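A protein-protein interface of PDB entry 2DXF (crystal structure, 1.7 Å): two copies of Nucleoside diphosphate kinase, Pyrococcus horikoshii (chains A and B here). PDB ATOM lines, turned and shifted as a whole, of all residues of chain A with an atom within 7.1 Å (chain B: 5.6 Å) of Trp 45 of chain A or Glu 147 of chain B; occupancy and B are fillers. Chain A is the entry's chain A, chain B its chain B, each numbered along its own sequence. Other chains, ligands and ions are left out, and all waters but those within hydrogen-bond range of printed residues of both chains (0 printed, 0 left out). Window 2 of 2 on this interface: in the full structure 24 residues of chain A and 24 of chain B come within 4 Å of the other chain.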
ATOM      1  N   PRO A  16      10.544  -1.505  30.758  1.00  0.00           N
ATOM      2  CA  PRO A  16      11.616  -1.885  29.837  1.00  0.00           C
ATOM      3  C   PRO A  16      12.773  -0.908  29.713  1.00  0.00           C
ATOM      4  O   PRO A  16      13.915  -1.333  29.583  1.00  0.00           O
ATOM      5  CB  PRO A  16      10.877  -2.097  28.517  1.00  0.00           C
ATOM      6  CG  PRO A  16       9.570  -2.628  28.974  1.00  0.00           C
ATOM      7  CD  PRO A  16       9.230  -1.704  30.120  1.00  0.00           C
ATOM      8  N   MET A  43      10.753 -11.168  37.540  1.00  0.00           N
ATOM      9  CA  MET A  43      10.983 -10.655  36.202  1.00  0.00           C
ATOM     10  C   MET A  43      10.099 -11.505  35.298  1.00  0.00           C
ATOM     11  O   MET A  43      10.138 -12.733  35.364  1.00  0.00           O
ATOM     12  CB  MET A  43      12.449 -10.817  35.788  1.00  0.00           C
ATOM     13  CG  MET A  43      12.699 -10.473  34.322  1.00  0.00           C
ATOM     14  SD  MET A  43      14.434 -10.481  33.837  1.00  0.00           S
ATOM     15  CE  MET A  43      14.918  -8.791  34.299  1.00  0.00           C
ATOM     16  N   ILE A  44       9.287 -10.843  34.480  1.00  0.00           N
ATOM     17  CA  ILE A  44       8.393 -11.520  33.547  1.00  0.00           C
ATOM     18  C   ILE A  44       8.420 -10.747  32.237  1.00  0.00           C
ATOM     19  O   ILE A  44       8.978  -9.650  32.167  1.00  0.00           O
ATOM     20  CB  ILE A  44       6.924 -11.527  34.054  1.00  0.00           C
ATOM     21  CG1 ILE A  44       6.428 -10.086  34.232  1.00  0.00           C
ATOM     22  CG2 ILE A  44       6.826 -12.298  35.363  1.00  0.00           C
ATOM     23  CD1 ILE A  44       4.953  -9.966  34.611  1.00  0.00           C
ATOM     24  N   TRP A  45       7.848 -11.330  31.190  1.00  0.00           N
ATOM     25  CA  TRP A  45       7.774 -10.631  29.915  1.00  0.00           C
ATOM     26  C   TRP A  45       6.282 -10.557  29.638  1.00  0.00           C
ATOM     27  O   TRP A  45       5.642 -11.562  29.325  1.00  0.00           O
ATOM     28  CB  TRP A  45       8.492 -11.386  28.793  1.00  0.00           C
ATOM     29  CG  TRP A  45       8.854 -10.484  27.641  1.00  0.00           C
ATOM     30  CD1 TRP A  45       8.140  -9.406  27.187  1.00  0.00           C
ATOM     31  CD2 TRP A  45      10.003 -10.586  26.788  1.00  0.00           C
ATOM     32  NE1 TRP A  45       8.773  -8.835  26.110  1.00  0.00           N
ATOM     33  CE2 TRP A  45       9.919  -9.538  25.842  1.00  0.00           C
ATOM     34  CE3 TRP A  45      11.098 -11.461  26.730  1.00  0.00           C
ATOM     35  CZ2 TRP A  45      10.887  -9.342  24.851  1.00  0.00           C
ATOM     36  CZ3 TRP A  45      12.063 -11.265  25.742  1.00  0.00           C
ATOM     37  CH2 TRP A  45      11.949 -10.211  24.817  1.00  0.00           C
ATOM     38  N   ILE A  46       5.733  -9.358  29.781  1.00  0.00           N
ATOM     39  CA  ILE A  46       4.309  -9.128  29.593  1.00  0.00           C
ATOM     40  C   ILE A  46       3.890  -9.202  28.134  1.00  0.00           C
ATOM     41  O   ILE A  46       4.521  -8.596  27.274  1.00  0.00           O
ATOM     42  CB  ILE A  46       3.912  -7.742  30.149  1.00  0.00           C
ATOM     43  CG1 ILE A  46       4.311  -7.639  31.626  1.00  0.00           C
ATOM     44  CG2 ILE A  46       2.413  -7.521  29.995  1.00  0.00           C
ATOM     45  CD1 ILE A  46       4.088  -6.264  32.238  1.00  0.00           C
ATOM     46  N   ASP A  47       2.832  -9.959  27.855  1.00  0.00           N
ATOM     47  CA  ASP A  47       2.334 -10.058  26.487  1.00  0.00           C
ATOM     48  C   ASP A  47       1.260  -8.993  26.314  1.00  0.00           C
ATOM     49  O   ASP A  47       0.834  -8.375  27.289  1.00  0.00           O
ATOM     50  CB  ASP A  47       1.765 -11.455  26.190  1.00  0.00           C
ATOM     51  CG  ASP A  47       0.664 -11.865  27.145  1.00  0.00           C
ATOM     52  OD1 ASP A  47      -0.247 -11.056  27.409  1.00  0.00           O
ATOM     53  OD2 ASP A  47       0.698 -13.019  27.624  1.00  0.00           O
ATOM     54  N   ARG A  48       0.822  -8.771  25.081  1.00  0.00           N
ATOM     55  CA  ARG A  48      -0.180  -7.744  24.828  1.00  0.00           C
ATOM     56  C   ARG A  48      -1.486  -7.913  25.597  1.00  0.00           C
ATOM     57  O   ARG A  48      -2.035  -6.935  26.101  1.00  0.00           O
ATOM     58  CB  ARG A  48      -0.466  -7.641  23.330  1.00  0.00           C
ATOM     59  CG  ARG A  48       0.769  -7.336  22.493  1.00  0.00           C
ATOM     60  CD  ARG A  48       0.399  -6.942  21.069  1.00  0.00           C
ATOM     61  NE  ARG A  48      -0.088  -5.565  20.984  1.00  0.00           N
ATOM     62  CZ  ARG A  48       0.697  -4.490  20.984  1.00  0.00           C
ATOM     63  NH1 ARG A  48       2.015  -4.625  21.061  1.00  0.00           N
ATOM     64  NH2 ARG A  48       0.165  -3.277  20.907  1.00  0.00           N
ATOM     65  N   LEU A  50      -2.089  -9.300  28.557  1.00  0.00           N
ATOM     66  CA  LEU A  50      -1.917  -8.919  29.952  1.00  0.00           C
ATOM     67  C   LEU A  50      -1.687  -7.414  30.070  1.00  0.00           C
ATOM     68  O   LEU A  50      -2.184  -6.772  30.997  1.00  0.00           O
ATOM     69  CB  LEU A  50      -0.735  -9.677  30.562  1.00  0.00           C
ATOM     70  CG  LEU A  50      -0.381  -9.355  32.016  1.00  0.00           C
ATOM     71  CD1 LEU A  50      -1.587  -9.596  32.914  1.00  0.00           C
ATOM     72  CD2 LEU A  50       0.795 -10.217  32.449  1.00  0.00           C
ATOM     73  N   ILE A  71       5.425  -1.230  27.130  1.00  0.00           N
ATOM     74  CA  ILE A  71       5.457  -2.114  28.292  1.00  0.00           C
ATOM     75  C   ILE A  71       5.781  -3.574  27.955  1.00  0.00           C
ATOM     76  O   ILE A  71       6.192  -4.333  28.831  1.00  0.00           O
ATOM     77  CB  ILE A  71       4.122  -2.031  29.091  1.00  0.00           C
ATOM     78  CG1 ILE A  71       4.360  -2.411  30.555  1.00  0.00           C
ATOM     79  CG2 ILE A  71       3.079  -2.954  28.485  1.00  0.00           C
ATOM     80  CD1 ILE A  71       5.224  -1.414  31.315  1.00  0.00           C
ATOM     81  N   THR A  72       5.615  -3.966  26.692  1.00  0.00           N
ATOM     82  CA  THR A  72       5.908  -5.345  26.287  1.00  0.00           C
ATOM     83  C   THR A  72       7.199  -5.450  25.479  1.00  0.00           C
ATOM     84  O   THR A  72       7.523  -6.518  24.955  1.00  0.00           O
ATOM     85  CB  THR A  72       4.773  -5.943  25.415  1.00  0.00           C
ATOM     86  OG1 THR A  72       4.718  -5.247  24.161  1.00  0.00           O
ATOM     87  CG2 THR A  72       3.431  -5.821  26.117  1.00  0.00           C
ATOM     88  N   LYS A  73       7.941  -4.349  25.391  1.00  0.00           N
ATOM     89  CA  LYS A  73       9.176  -4.306  24.610  1.00  0.00           C
ATOM     90  C   LYS A  73      10.254  -5.300  25.050  1.00  0.00           C
ATOM     91  O   LYS A  73      10.888  -5.945  24.212  1.00  0.00           O
ATOM     92  CB  LYS A  73       9.740  -2.884  24.623  1.00  0.00           C
ATOM     93  CG  LYS A  73      10.797  -2.623  23.566  1.00  0.00           C
ATOM     94  CD  LYS A  73      11.164  -1.148  23.528  1.00  0.00           C
ATOM     95  CE  LYS A  73      12.214  -0.848  22.472  1.00  0.00           C
ATOM     96  NZ  LYS A  73      11.699  -1.042  21.090  1.00  0.00           N
ATOM     97  N   THR A  74      10.465  -5.407  26.358  1.00  0.00           N
ATOM     98  CA  THR A  74      11.447  -6.338  26.917  1.00  0.00           C
ATOM     99  C   THR A  74      10.886  -6.820  28.246  1.00  0.00           C
ATOM    100  O   THR A  74       9.810  -6.396  28.665  1.00  0.00           O
ATOM    101  CB  THR A  74      12.808  -5.662  27.229  1.00  0.00           C
ATOM    102  OG1 THR A  74      12.656  -4.792  28.358  1.00  0.00           O
ATOM    103  CG2 THR A  74      13.317  -4.873  26.044  1.00  0.00           C
ATOM    104  N   PRO A  75      11.599  -7.734  28.922  1.00  0.00           N
ATOM    105  CA  PRO A  75      11.070  -8.188  30.208  1.00  0.00           C
ATOM    106  C   PRO A  75      11.044  -6.997  31.164  1.00  0.00           C
ATOM    107  O   PRO A  75      11.745  -6.005  30.946  1.00  0.00           O
ATOM    108  CB  PRO A  75      12.087  -9.243  30.641  1.00  0.00           C
ATOM    109  CG  PRO A  75      12.537  -9.814  29.345  1.00  0.00           C
ATOM    110  CD  PRO A  75      12.708  -8.592  28.474  1.00  0.00           C
ATOM    111  N   VAL A  76      10.224  -7.097  32.203  1.00  0.00           N
ATOM    112  CA  VAL A  76      10.116  -6.045  33.207  1.00  0.00           C
ATOM    113  C   VAL A  76      10.193  -6.729  34.563  1.00  0.00           C
ATOM    114  O   VAL A  76      10.223  -7.957  34.643  1.00  0.00           O
ATOM    115  CB  VAL A  76       8.757  -5.305  33.130  1.00  0.00           C
ATOM    116  CG1 VAL A  76       8.630  -4.575  31.806  1.00  0.00           C
ATOM    117  CG2 VAL A  76       7.610  -6.299  33.302  1.00  0.00           C
ATOM    118  N   ARG B   9      25.895 -18.550  32.158  1.00  0.00           N
ATOM    119  CA  ARG B   9      24.805 -18.175  33.051  1.00  0.00           C
ATOM    120  C   ARG B   9      25.110 -18.754  34.425  1.00  0.00           C
ATOM    121  O   ARG B   9      25.469 -19.928  34.549  1.00  0.00           O
ATOM    122  CB  ARG B   9      23.467 -18.734  32.562  1.00  0.00           C
ATOM    123  CG  ARG B   9      22.879 -18.027  31.348  1.00  0.00           C
ATOM    124  CD  ARG B   9      21.523 -18.618  30.995  1.00  0.00           C
ATOM    125  NE  ARG B   9      20.864 -17.875  29.926  1.00  0.00           N
ATOM    126  CZ  ARG B   9      19.648 -18.151  29.469  1.00  0.00           C
ATOM    127  NH1 ARG B   9      18.957 -19.157  29.989  1.00  0.00           N
ATOM    128  NH2 ARG B   9      19.119 -17.417  28.498  1.00  0.00           N
ATOM    129  N   LEU B 145      13.143 -17.642  32.069  1.00  0.00           N
ATOM    130  CA  LEU B 145      14.438 -17.107  31.654  1.00  0.00           C
ATOM    131  C   LEU B 145      14.251 -16.423  30.311  1.00  0.00           C
ATOM    132  O   LEU B 145      13.649 -16.990  29.398  1.00  0.00           O
ATOM    133  CB  LEU B 145      15.466 -18.235  31.554  1.00  0.00           C
ATOM    134  CG  LEU B 145      15.639 -19.037  32.849  1.00  0.00           C
ATOM    135  CD1 LEU B 145      16.679 -20.124  32.656  1.00  0.00           C
ATOM    136  CD2 LEU B 145      16.047 -18.096  33.980  1.00  0.00           C
ATOM    137  N   PHE B 146      14.782 -15.212  30.178  1.00  0.00           N
ATOM    138  CA  PHE B 146      14.586 -14.459  28.948  1.00  0.00           C
ATOM    139  C   PHE B 146      15.814 -14.032  28.163  1.00  0.00           C
ATOM    140  O   PHE B 146      16.913 -13.887  28.702  1.00  0.00           O
ATOM    141  CB  PHE B 146      13.741 -13.221  29.253  1.00  0.00           C
ATOM    142  CG  PHE B 146      12.567 -13.499  30.142  1.00  0.00           C
ATOM    143  CD1 PHE B 146      12.651 -13.287  31.514  1.00  0.00           C
ATOM    144  CD2 PHE B 146      11.382 -14.001  29.613  1.00  0.00           C
ATOM    145  CE1 PHE B 146      11.570 -13.572  32.350  1.00  0.00           C
ATOM    146  CE2 PHE B 146      10.298 -14.290  30.439  1.00  0.00           C
ATOM    147  CZ  PHE B 146      10.392 -14.075  31.811  1.00  0.00           C
ATOM    148  N   GLU B 147      15.596 -13.830  26.868  1.00  0.00           N
ATOM    149  CA  GLU B 147      16.632 -13.386  25.947  1.00  0.00           C
ATOM    150  C   GLU B 147      16.184 -12.016  25.443  1.00  0.00           C
ATOM    151  O   GLU B 147      15.176 -11.905  24.749  1.00  0.00           O
ATOM    152  CB  GLU B 147      16.755 -14.364  24.777  1.00  0.00           C
ATOM    153  CG  GLU B 147      17.912 -14.068  23.840  1.00  0.00           C
ATOM    154  CD  GLU B 147      18.060 -15.115  22.752  1.00  0.00           C
ATOM    155  OE1 GLU B 147      18.213 -16.306  23.094  1.00  0.00           O
ATOM    156  OE2 GLU B 147      18.021 -14.747  21.559  1.00  0.00           O
ATOM    157  N   TYR B 148      16.925 -10.976  25.807  1.00  0.00           N
ATOM    158  CA  TYR B 148      16.575  -9.618  25.404  1.00  0.00           C
ATOM    159  C   TYR B 148      17.830  -8.761  25.409  1.00  0.00           C
ATOM    160  O   TYR B 148      18.827  -9.103  26.044  1.00  0.00           O
ATOM    161  CB  TYR B 148      15.539  -9.040  26.370  1.00  0.00           C
ATOM    162  CG  TYR B 148      16.083  -8.807  27.758  1.00  0.00           C
ATOM    163  CD1 TYR B 148      16.621  -7.572  28.119  1.00  0.00           C
ATOM    164  CD2 TYR B 148      16.095  -9.833  28.700  1.00  0.00           C
ATOM    165  CE1 TYR B 148      17.162  -7.366  29.388  1.00  0.00           C
ATOM    166  CE2 TYR B 148      16.633  -9.640  29.967  1.00  0.00           C
ATOM    167  CZ  TYR B 148      17.164  -8.405  30.305  1.00  0.00           C
ATOM    168  OH  TYR B 148      17.701  -8.219  31.559  1.00  0.00           O
ATOM    169  N   PRO B 149      17.796  -7.622  24.707  1.00  0.00           N
ATOM    170  CA  PRO B 149      18.976  -6.761  24.669  1.00  0.00           C
ATOM    171  C   PRO B 149      19.104  -5.740  25.793  1.00  0.00           C
ATOM    172  O   PRO B 149      18.130  -5.093  26.171  1.00  0.00           O
ATOM    173  CB  PRO B 149      18.847  -6.082  23.313  1.00  0.00           C
ATOM    174  CG  PRO B 149      17.366  -5.867  23.216  1.00  0.00           C
ATOM    175  CD  PRO B 149      16.793  -7.187  23.715  1.00  0.00           C
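Among the printed residues, pairs that only touch across the chains: Trp 45 of chain A with Glu 147 of chain B, Met 43 of chain A with Phe 146 of chain B, Pro 75 of chain A with Tyr 148 of chain B, Pro 75 of chain A with Phe 146 of chain B, Ile 44 of chain A with Phe 146 of chain B, Trp 45 of chain A with Phe 146 of chain B and Met 43 of chain A with Tyr 148 of chain B.
The backbone NH (N) of Val 76 of chain A is in hydrogen-bond range of the backbone carbonyl oxygen (O) of Ile 44 of chain A (2.8 Å).
The indole nitrogen (NE1) of Trp 45 of chain A sits at hydrogen-bond distance from the backbone carbonyl oxygen (O) of Thr 72 of chain A.
No position is printed for both chains.
Of the 7 pairs that touch across the chains among the printed residues, none has its exchanged pair printed and touching as well.
Of the 6 printed residues of chain B, 3 touch a printed residue of chain A.
Printed residues of chain B that touch a printed residue of chain A: Phe 146, Glu 147 and Tyr 148.
Among the printed residues, no Asp or Glu carboxylate lies within 4 Å of a Lys or Arg side-chain nitrogen of the other chain.
Of chain B, only Phe 146 and Glu 147 come within 4 Å of Trp 45 of chain A.
Glu 147 of chain B touches just one residue of chain A: Trp 45 (3.3 Å).
Of the printed residues of chain B, Pro 75 of chain A touches Phe 146 (3.6 Å) and Tyr 148 (3.5 Å).
Printed residues of chain A within 4 Å of Phe 146 of chain B: Met 43 (3.4 Å), Ile 44 (3.7 Å), Trp 45 (3.8 Å) and Pro 75 (3.6 Å).
Of the printed residues of chain B, Ile 44 of chain A touches Phe 146.
Of the printed residues of chain A, Tyr 148 of chain B touches Met 43 (3.9 Å) and Pro 75 (3.5 Å).
Printed residues of chain B within 4 Å of Met 43 of chain A: Phe 146 and Tyr 148.
The nearest residue of chain B that does not touch Trp 45 of chain A is Tyr 148 of chain B (4.1 Å).
The nearest printed residue of chain A that does not touch Phe 146 of chain B is Val 76 of chain A (6.2 Å).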
